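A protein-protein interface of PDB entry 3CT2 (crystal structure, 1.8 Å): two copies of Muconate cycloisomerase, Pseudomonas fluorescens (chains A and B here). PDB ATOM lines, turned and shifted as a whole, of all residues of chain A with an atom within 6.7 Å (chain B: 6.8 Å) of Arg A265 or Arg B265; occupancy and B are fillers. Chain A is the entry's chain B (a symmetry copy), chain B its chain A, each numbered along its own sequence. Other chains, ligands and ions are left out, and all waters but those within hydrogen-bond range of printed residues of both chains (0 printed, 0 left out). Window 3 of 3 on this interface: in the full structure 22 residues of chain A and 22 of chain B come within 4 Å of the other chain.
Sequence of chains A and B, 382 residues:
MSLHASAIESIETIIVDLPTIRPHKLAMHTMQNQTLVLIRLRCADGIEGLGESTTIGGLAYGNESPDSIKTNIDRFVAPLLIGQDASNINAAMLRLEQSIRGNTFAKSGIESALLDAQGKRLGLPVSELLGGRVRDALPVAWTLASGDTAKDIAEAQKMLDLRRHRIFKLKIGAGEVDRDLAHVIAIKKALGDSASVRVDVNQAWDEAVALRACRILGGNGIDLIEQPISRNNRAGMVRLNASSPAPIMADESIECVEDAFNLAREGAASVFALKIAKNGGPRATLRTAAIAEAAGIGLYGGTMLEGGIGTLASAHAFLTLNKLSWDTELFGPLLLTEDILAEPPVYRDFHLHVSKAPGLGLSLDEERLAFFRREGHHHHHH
Among the printed residues, merely in contact across the chains: Phe A261 with Phe B261 (3.8 Å), Phe A261 with Ala B264 (3.6 Å), Phe A261 with Arg B265 (3.97 Å), Phe A261 with Ala B295 (3.5 Å), Ala A264 with Phe B261 (3.6 Å), Arg A265 with Arg B265 (3.9 Å) and Ala A295 with Phe B261 (3.4 Å).
The side-chain amide nitrogen (ND2) of Asn A262 sits close to the guanidinium group (NH2) of Arg A265 (3.1 Å).
The side-chain amide nitrogen (ND2) of Asn B262 lies close to the guanidinium group (NH2) of Arg B265 (3.2 Å).
Phe B261 touches its own counterpart, Phe A261.
Phe A261 touches Arg B265, but with the chains exchanged Arg A265 does not touch Phe B261 (4.05 Å).
Phe A261 touches Ala B295, and with the chains exchanged Ala A295 touches Phe B261.
Arg A265 touches its own counterpart, Arg B265.
14 positions are printed for both chains.
Of the 14 printed residues of chain B, 4 touch a printed residue of chain A.
Hydrophobic or aromatic side chains of chain B that line the printed part of chain A: Phe B261, Ala B264 and Ala B295.
Among the printed residues, no Asp or Glu carboxylate lies within 4 Å of a Lys or Arg side-chain nitrogen of the other chain.
Arg A234 touches none of the printed residues of chain B.
Arg A265 touches just one residue of chain B: Arg B265 (3.9 Å).
Of the printed residues of chain B, Ala A295 touches Phe B261.
Printed residues of chain A within 4 Å of Phe B261: Phe A261, Ala A264 and Ala A295.
Of the printed residues of chain A, Ala B264 touches Phe A261 (3.6 Å).
Of the printed residues of chain A, Arg B265 touches Phe A261 (3.97 Å) and Arg A265 (3.9 Å).
The nearest printed residue of chain A that does not touch Ala B295 is Asn A262 (6.4 Å).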
ATOM      1  N   ARG A 234      11.495 -14.051 -14.878  1.00  0.00           N
ATOM      2  CA  ARG A 234      11.805 -13.930 -16.297  1.00  0.00           C
ATOM      3  C   ARG A 234      10.603 -13.560 -17.154  1.00  0.00           C
ATOM      4  O   ARG A 234      10.679 -12.660 -17.988  1.00  0.00           O
ATOM      5  CB  ARG A 234      12.423 -15.242 -16.797  1.00  0.00           C
ATOM      6  CG  ARG A 234      13.585 -15.732 -15.935  1.00  0.00           C
ATOM      7  CD  ARG A 234      14.237 -16.974 -16.543  1.00  0.00           C
ATOM      8  NE  ARG A 234      14.876 -16.664 -17.819  1.00  0.00           N
ATOM      9  CZ  ARG A 234      16.129 -16.239 -17.948  1.00  0.00           C
ATOM     10  NH1 ARG A 234      16.898 -16.084 -16.882  1.00  0.00           N
ATOM     11  NH2 ARG A 234      16.603 -15.943 -19.145  1.00  0.00           N
ATOM     12  N   ASP A 259      23.503 -14.747 -20.474  1.00  0.00           N
ATOM     13  CA  ASP A 259      22.267 -14.158 -19.962  1.00  0.00           C
ATOM     14  C   ASP A 259      21.798 -13.096 -20.942  1.00  0.00           C
ATOM     15  O   ASP A 259      20.597 -12.940 -21.178  1.00  0.00           O
ATOM     16  CB  ASP A 259      22.486 -13.507 -18.593  1.00  0.00           C
ATOM     17  CG  ASP A 259      22.569 -14.518 -17.467  1.00  0.00           C
ATOM     18  OD1 ASP A 259      22.158 -15.687 -17.662  1.00  0.00           O
ATOM     19  OD2 ASP A 259      23.031 -14.137 -16.371  1.00  0.00           O
ATOM     20  N   ALA A 260      22.750 -12.363 -21.511  1.00  0.00           N
ATOM     21  CA  ALA A 260      22.428 -11.313 -22.472  1.00  0.00           C
ATOM     22  C   ALA A 260      21.661 -11.900 -23.650  1.00  0.00           C
ATOM     23  O   ALA A 260      20.639 -11.353 -24.069  1.00  0.00           O
ATOM     24  CB  ALA A 260      23.706 -10.633 -22.960  1.00  0.00           C
ATOM     25  N   PHE A 261      22.148 -13.015 -24.187  1.00  0.00           N
ATOM     26  CA  PHE A 261      21.456 -13.627 -25.305  1.00  0.00           C
ATOM     27  C   PHE A 261      20.050 -14.063 -24.914  1.00  0.00           C
ATOM     28  O   PHE A 261      19.092 -13.781 -25.626  1.00  0.00           O
ATOM     29  CB  PHE A 261      22.201 -14.849 -25.851  1.00  0.00           C
ATOM     30  CG  PHE A 261      21.371 -15.649 -26.806  1.00  0.00           C
ATOM     31  CD1 PHE A 261      21.077 -15.149 -28.075  1.00  0.00           C
ATOM     32  CD2 PHE A 261      20.780 -16.842 -26.400  1.00  0.00           C
ATOM     33  CE1 PHE A 261      20.199 -15.820 -28.920  1.00  0.00           C
ATOM     34  CE2 PHE A 261      19.897 -17.523 -27.241  1.00  0.00           C
ATOM     35  CZ  PHE A 261      19.604 -17.009 -28.502  1.00  0.00           C
ATOM     36  N   ASN A 262      19.927 -14.759 -23.789  1.00  0.00           N
ATOM     37  CA  ASN A 262      18.616 -15.225 -23.356  1.00  0.00           C
ATOM     38  C   ASN A 262      17.641 -14.077 -23.124  1.00  0.00           C
ATOM     39  O   ASN A 262      16.468 -14.179 -23.490  1.00  0.00           O
ATOM     40  CB  ASN A 262      18.749 -16.100 -22.109  1.00  0.00           C
ATOM     41  CG  ASN A 262      19.266 -17.491 -22.437  1.00  0.00           C
ATOM     42  OD1 ASN A 262      20.253 -17.948 -21.866  1.00  0.00           O
ATOM     43  ND2 ASN A 262      18.594 -18.169 -23.365  1.00  0.00           N
ATOM     44  N   LEU A 263      18.116 -12.984 -22.533  1.00  0.00           N
ATOM     45  CA  LEU A 263      17.251 -11.831 -22.302  1.00  0.00           C
ATOM     46  C   LEU A 263      16.778 -11.244 -23.635  1.00  0.00           C
ATOM     47  O   LEU A 263      15.622 -10.867 -23.777  1.00  0.00           O
ATOM     48  CB  LEU A 263      17.991 -10.759 -21.498  1.00  0.00           C
ATOM     49  CG  LEU A 263      18.360 -11.126 -20.056  1.00  0.00           C
ATOM     50  CD1 LEU A 263      19.166  -9.989 -19.433  1.00  0.00           C
ATOM     51  CD2 LEU A 263      17.091 -11.396 -19.249  1.00  0.00           C
ATOM     52  N   ALA A 264      17.679 -11.159 -24.610  1.00  0.00           N
ATOM     53  CA  ALA A 264      17.317 -10.630 -25.922  1.00  0.00           C
ATOM     54  C   ALA A 264      16.340 -11.581 -26.614  1.00  0.00           C
ATOM     55  O   ALA A 264      15.387 -11.151 -27.261  1.00  0.00           O
ATOM     56  CB  ALA A 264      18.572 -10.438 -26.779  1.00  0.00           C
ATOM     57  N   ARG A 265      16.576 -12.881 -26.482  1.00  0.00           N
ATOM     58  CA  ARG A 265      15.682 -13.870 -27.089  1.00  0.00           C
ATOM     59  C   ARG A 265      14.266 -13.744 -26.531  1.00  0.00           C
ATOM     60  O   ARG A 265      13.283 -13.754 -27.280  1.00  0.00           O
ATOM     61  CB  ARG A 265      16.201 -15.288 -26.822  1.00  0.00           C
ATOM     62  CG  ARG A 265      15.282 -16.411 -27.330  1.00  0.00           C
ATOM     63  CD  ARG A 265      15.900 -17.777 -27.031  1.00  0.00           C
ATOM     64  NE  ARG A 265      16.128 -17.949 -25.600  1.00  0.00           N
ATOM     65  CZ  ARG A 265      15.173 -18.246 -24.723  1.00  0.00           C
ATOM     66  NH1 ARG A 265      13.921 -18.418 -25.132  1.00  0.00           N
ATOM     67  NH2 ARG A 265      15.466 -18.358 -23.436  1.00  0.00           N
ATOM     68  N   GLU A 266      14.163 -13.609 -25.215  1.00  0.00           N
ATOM     69  CA  GLU A 266      12.858 -13.517 -24.565  1.00  0.00           C
ATOM     70  C   GLU A 266      12.175 -12.172 -24.718  1.00  0.00           C
ATOM     71  O   GLU A 266      10.949 -12.100 -24.678  1.00  0.00           O
ATOM     72  CB  GLU A 266      12.987 -13.785 -23.072  1.00  0.00           C
ATOM     73  CG  GLU A 266      13.570 -15.112 -22.682  1.00  0.00           C
ATOM     74  CD  GLU A 266      13.797 -15.158 -21.184  1.00  0.00           C
ATOM     75  OE1 GLU A 266      14.555 -14.298 -20.671  1.00  0.00           O
ATOM     76  OE2 GLU A 266      13.210 -16.028 -20.519  1.00  0.00           O
ATOM     77  N   GLY A 267      12.974 -11.118 -24.861  1.00  0.00           N
ATOM     78  CA  GLY A 267      12.436  -9.768 -24.967  1.00  0.00           C
ATOM     79  C   GLY A 267      12.240  -9.212 -23.562  1.00  0.00           C
ATOM     80  O   GLY A 267      11.236  -8.552 -23.281  1.00  0.00           O
ATOM     81  N   ALA A 268      13.207  -9.466 -22.681  1.00  0.00           N
ATOM     82  CA  ALA A 268      13.129  -9.030 -21.282  1.00  0.00           C
ATOM     83  C   ALA A 268      13.489  -7.577 -20.977  1.00  0.00           C
ATOM     84  O   ALA A 268      13.202  -7.092 -19.881  1.00  0.00           O
ATOM     85  CB  ALA A 268      13.977  -9.941 -20.417  1.00  0.00           C
ATOM     86  N   PHE A 272      20.347  -2.691 -22.267  1.00  0.00           N
ATOM     87  CA  PHE A 272      21.193  -3.522 -21.404  1.00  0.00           C
ATOM     88  C   PHE A 272      22.278  -2.678 -20.754  1.00  0.00           C
ATOM     89  O   PHE A 272      22.933  -1.880 -21.431  1.00  0.00           O
ATOM     90  CB  PHE A 272      21.943  -4.608 -22.195  1.00  0.00           C
ATOM     91  CG  PHE A 272      21.108  -5.788 -22.612  1.00  0.00           C
ATOM     92  CD1 PHE A 272      19.782  -5.921 -22.216  1.00  0.00           C
ATOM     93  CD2 PHE A 272      21.678  -6.789 -23.408  1.00  0.00           C
ATOM     94  CE1 PHE A 272      19.029  -7.035 -22.607  1.00  0.00           C
ATOM     95  CE2 PHE A 272      20.934  -7.905 -23.803  1.00  0.00           C
ATOM     96  CZ  PHE A 272      19.607  -8.026 -23.401  1.00  0.00           C
ATOM     97  N   ALA A 295      20.492  -7.521 -31.628  1.00  0.00           N
ATOM     98  CA  ALA A 295      19.083  -7.674 -31.282  1.00  0.00           C
ATOM     99  C   ALA A 295      18.323  -6.348 -31.298  1.00  0.00           C
ATOM    100  O   ALA A 295      17.112  -6.326 -31.065  1.00  0.00           O
ATOM    101  CB  ALA A 295      18.951  -8.330 -29.897  1.00  0.00           C
ATOM    102  N   ILE A 297      18.932  -3.872 -29.235  1.00  0.00           N
ATOM    103  CA  ILE A 297      18.819  -3.433 -27.848  1.00  0.00           C
ATOM    104  C   ILE A 297      19.814  -2.310 -27.549  1.00  0.00           C
ATOM    105  O   ILE A 297      20.981  -2.384 -27.941  1.00  0.00           O
ATOM    106  CB  ILE A 297      19.048  -4.642 -26.899  1.00  0.00           C
ATOM    107  CG1 ILE A 297      17.892  -5.633 -27.071  1.00  0.00           C
ATOM    108  CG2 ILE A 297      19.159  -4.179 -25.449  1.00  0.00           C
ATOM    109  CD1 ILE A 297      18.067  -6.945 -26.325  1.00  0.00           C
ATOM    110  N   ARG B 234      11.540 -19.368 -42.819  1.00  0.00           N
ATOM    111  CA  ARG B 234      12.019 -19.226 -41.451  1.00  0.00           C
ATOM    112  C   ARG B 234      11.362 -20.195 -40.479  1.00  0.00           C
ATOM    113  O   ARG B 234      12.045 -20.848 -39.692  1.00  0.00           O
ATOM    114  CB  ARG B 234      11.806 -17.782 -40.983  1.00  0.00           C
ATOM    115  CG  ARG B 234      12.359 -16.733 -41.950  1.00  0.00           C
ATOM    116  CD  ARG B 234      12.214 -15.317 -41.387  1.00  0.00           C
ATOM    117  NE  ARG B 234      13.045 -15.135 -40.203  1.00  0.00           N
ATOM    118  CZ  ARG B 234      14.314 -14.741 -40.227  1.00  0.00           C
ATOM    119  NH1 ARG B 234      14.911 -14.468 -41.380  1.00  0.00           N
ATOM    120  NH2 ARG B 234      15.000 -14.651 -39.094  1.00  0.00           N
ATOM    121  N   ASP B 259      21.395 -11.529 -38.610  1.00  0.00           N
ATOM    122  CA  ASP B 259      20.692 -12.749 -38.996  1.00  0.00           C
ATOM    123  C   ASP B 259      21.053 -13.842 -38.002  1.00  0.00           C
ATOM    124  O   ASP B 259      20.217 -14.667 -37.634  1.00  0.00           O
ATOM    125  CB  ASP B 259      21.100 -13.202 -40.404  1.00  0.00           C
ATOM    126  CG  ASP B 259      20.453 -12.378 -41.498  1.00  0.00           C
ATOM    127  OD1 ASP B 259      19.467 -11.655 -41.218  1.00  0.00           O
ATOM    128  OD2 ASP B 259      20.925 -12.467 -42.645  1.00  0.00           O
ATOM    129  N   ALA B 260      22.310 -13.852 -37.574  1.00  0.00           N
ATOM    130  CA  ALA B 260      22.774 -14.855 -36.628  1.00  0.00           C
ATOM    131  C   ALA B 260      21.946 -14.779 -35.353  1.00  0.00           C
ATOM    132  O   ALA B 260      21.489 -15.802 -34.834  1.00  0.00           O
ATOM    133  CB  ALA B 260      24.248 -14.640 -36.317  1.00  0.00           C
ATOM    134  N   PHE B 261      21.745 -13.570 -34.840  1.00  0.00           N
ATOM    135  CA  PHE B 261      20.952 -13.442 -33.633  1.00  0.00           C
ATOM    136  C   PHE B 261      19.522 -13.932 -33.843  1.00  0.00           C
ATOM    137  O   PHE B 261      18.998 -14.697 -33.032  1.00  0.00           O
ATOM    138  CB  PHE B 261      20.888 -11.999 -33.136  1.00  0.00           C
ATOM    139  CG  PHE B 261      19.863 -11.806 -32.064  1.00  0.00           C
ATOM    140  CD1 PHE B 261      20.065 -12.334 -30.793  1.00  0.00           C
ATOM    141  CD2 PHE B 261      18.645 -11.192 -32.352  1.00  0.00           C
ATOM    142  CE1 PHE B 261      19.067 -12.260 -29.819  1.00  0.00           C
ATOM    143  CE2 PHE B 261      17.645 -11.113 -31.389  1.00  0.00           C
ATOM    144  CZ  PHE B 261      17.858 -11.650 -30.119  1.00  0.00           C
ATOM    145  N   ASN B 262      18.885 -13.488 -34.924  1.00  0.00           N
ATOM    146  CA  ASN B 262      17.510 -13.892 -35.184  1.00  0.00           C
ATOM    147  C   ASN B 262      17.378 -15.400 -35.344  1.00  0.00           C
ATOM    148  O   ASN B 262      16.418 -15.995 -34.846  1.00  0.00           O
ATOM    149  CB  ASN B 262      16.954 -13.154 -36.408  1.00  0.00           C
ATOM    150  CG  ASN B 262      16.603 -11.701 -36.098  1.00  0.00           C
ATOM    151  OD1 ASN B 262      17.062 -10.779 -36.768  1.00  0.00           O
ATOM    152  ND2 ASN B 262      15.780 -11.500 -35.076  1.00  0.00           N
ATOM    153  N   LEU B 263      18.340 -16.028 -36.018  1.00  0.00           N
ATOM    154  CA  LEU B 263      18.293 -17.480 -36.191  1.00  0.00           C
ATOM    155  C   LEU B 263      18.410 -18.177 -34.834  1.00  0.00           C
ATOM    156  O   LEU B 263      17.704 -19.148 -34.561  1.00  0.00           O
ATOM    157  CB  LEU B 263      19.427 -17.955 -37.111  1.00  0.00           C
ATOM    158  CG  LEU B 263      19.341 -17.496 -38.571  1.00  0.00           C
ATOM    159  CD1 LEU B 263      20.583 -17.959 -39.321  1.00  0.00           C
ATOM    160  CD2 LEU B 263      18.072 -18.049 -39.220  1.00  0.00           C
ATOM    161  N   ALA B 264      19.296 -17.677 -33.980  1.00  0.00           N
ATOM    162  CA  ALA B 264      19.469 -18.263 -32.652  1.00  0.00           C
ATOM    163  C   ALA B 264      18.196 -18.055 -31.824  1.00  0.00           C
ATOM    164  O   ALA B 264      17.764 -18.948 -31.102  1.00  0.00           O
ATOM    165  CB  ALA B 264      20.657 -17.628 -31.950  1.00  0.00           C
ATOM    166  N   ARG B 265      17.604 -16.870 -31.925  1.00  0.00           N
ATOM    167  CA  ARG B 265      16.375 -16.570 -31.187  1.00  0.00           C
ATOM    168  C   ARG B 265      15.254 -17.527 -31.580  1.00  0.00           C
ATOM    169  O   ARG B 265      14.547 -18.071 -30.727  1.00  0.00           O
ATOM    170  CB  ARG B 265      15.925 -15.128 -31.473  1.00  0.00           C
ATOM    171  CG  ARG B 265      14.589 -14.729 -30.819  1.00  0.00           C
ATOM    172  CD  ARG B 265      14.263 -13.268 -31.131  1.00  0.00           C
ATOM    173  NE  ARG B 265      14.179 -13.053 -32.572  1.00  0.00           N
ATOM    174  CZ  ARG B 265      13.138 -13.404 -33.321  1.00  0.00           C
ATOM    175  NH1 ARG B 265      12.079 -13.981 -32.765  1.00  0.00           N
ATOM    176  NH2 ARG B 265      13.163 -13.197 -34.628  1.00  0.00           N
ATOM    177  N   GLU B 266      15.095 -17.737 -32.879  1.00  0.00           N
ATOM    178  CA  GLU B 266      14.040 -18.605 -33.382  1.00  0.00           C
ATOM    179  C   GLU B 266      14.304 -20.089 -33.201  1.00  0.00           C
ATOM    180  O   GLU B 266      13.362 -20.874 -33.093  1.00  0.00           O
ATOM    181  CB  GLU B 266      13.823 -18.371 -34.873  1.00  0.00           C
ATOM    182  CG  GLU B 266      13.478 -16.968 -35.279  1.00  0.00           C
ATOM    183  CD  GLU B 266      13.452 -16.858 -36.789  1.00  0.00           C
ATOM    184  OE1 GLU B 266      14.494 -17.148 -37.424  1.00  0.00           O
ATOM    185  OE2 GLU B 266      12.395 -16.505 -37.341  1.00  0.00           O
ATOM    186  N   GLY B 267      15.580 -20.468 -33.193  1.00  0.00           N
ATOM    187  CA  GLY B 267      15.946 -21.871 -33.075  1.00  0.00           C
ATOM    188  C   GLY B 267      15.948 -22.486 -34.469  1.00  0.00           C
ATOM    189  O   GLY B 267      15.479 -23.607 -34.663  1.00  0.00           O
ATOM    190  N   ALA B 268      16.490 -21.756 -35.442  1.00  0.00           N
ATOM    191  CA  ALA B 268      16.516 -22.209 -36.834  1.00  0.00           C
ATOM    192  C   ALA B 268      17.624 -23.181 -37.223  1.00  0.00           C
ATOM    193  O   ALA B 268      17.555 -23.795 -38.291  1.00  0.00           O
ATOM    194  CB  ALA B 268      16.557 -21.000 -37.769  1.00  0.00           C
ATOM    195  N   PHE B 272      26.125 -23.064 -36.903  1.00  0.00           N
ATOM    196  CA  PHE B 272      26.218 -21.929 -37.826  1.00  0.00           C
ATOM    197  C   PHE B 272      27.517 -22.005 -38.621  1.00  0.00           C
ATOM    198  O   PHE B 272      28.580 -22.249 -38.050  1.00  0.00           O
ATOM    199  CB  PHE B 272      26.274 -20.578 -37.093  1.00  0.00           C
ATOM    200  CG  PHE B 272      24.960 -20.095 -36.543  1.00  0.00           C
ATOM    201  CD1 PHE B 272      23.776 -20.787 -36.765  1.00  0.00           C
ATOM    202  CD2 PHE B 272      24.922 -18.916 -35.793  1.00  0.00           C
ATOM    203  CE1 PHE B 272      22.565 -20.310 -36.245  1.00  0.00           C
ATOM    204  CE2 PHE B 272      23.724 -18.434 -35.271  1.00  0.00           C
ATOM    205  CZ  PHE B 272      22.543 -19.135 -35.499  1.00  0.00           C
ATOM    206  N   ALA B 295      24.486 -18.690 -27.455  1.00  0.00           N
ATOM    207  CA  ALA B 295      23.230 -19.410 -27.634  1.00  0.00           C
ATOM    208  C   ALA B 295      23.403 -20.929 -27.578  1.00  0.00           C
ATOM    209  O   ALA B 295      22.420 -21.673 -27.690  1.00  0.00           O
ATOM    210  CB  ALA B 295      22.590 -19.016 -28.969  1.00  0.00           C
ATOM    211  N   ILE B 297      25.092 -22.651 -29.773  1.00  0.00           N
ATOM    212  CA  ILE B 297      25.103 -23.125 -31.152  1.00  0.00           C
ATOM    213  C   ILE B 297      26.526 -23.464 -31.609  1.00  0.00           C
ATOM    214  O   ILE B 297      27.464 -22.705 -31.353  1.00  0.00           O
ATOM    215  CB  ILE B 297      24.473 -22.055 -32.081  1.00  0.00           C
ATOM    216  CG1 ILE B 297      22.981 -21.908 -31.733  1.00  0.00           C
ATOM    217  CG2 ILE B 297      24.648 -22.447 -33.547  1.00  0.00           C
ATOM    218  CD1 ILE B 297      22.264 -20.780 -32.474  1.00  0.00           C
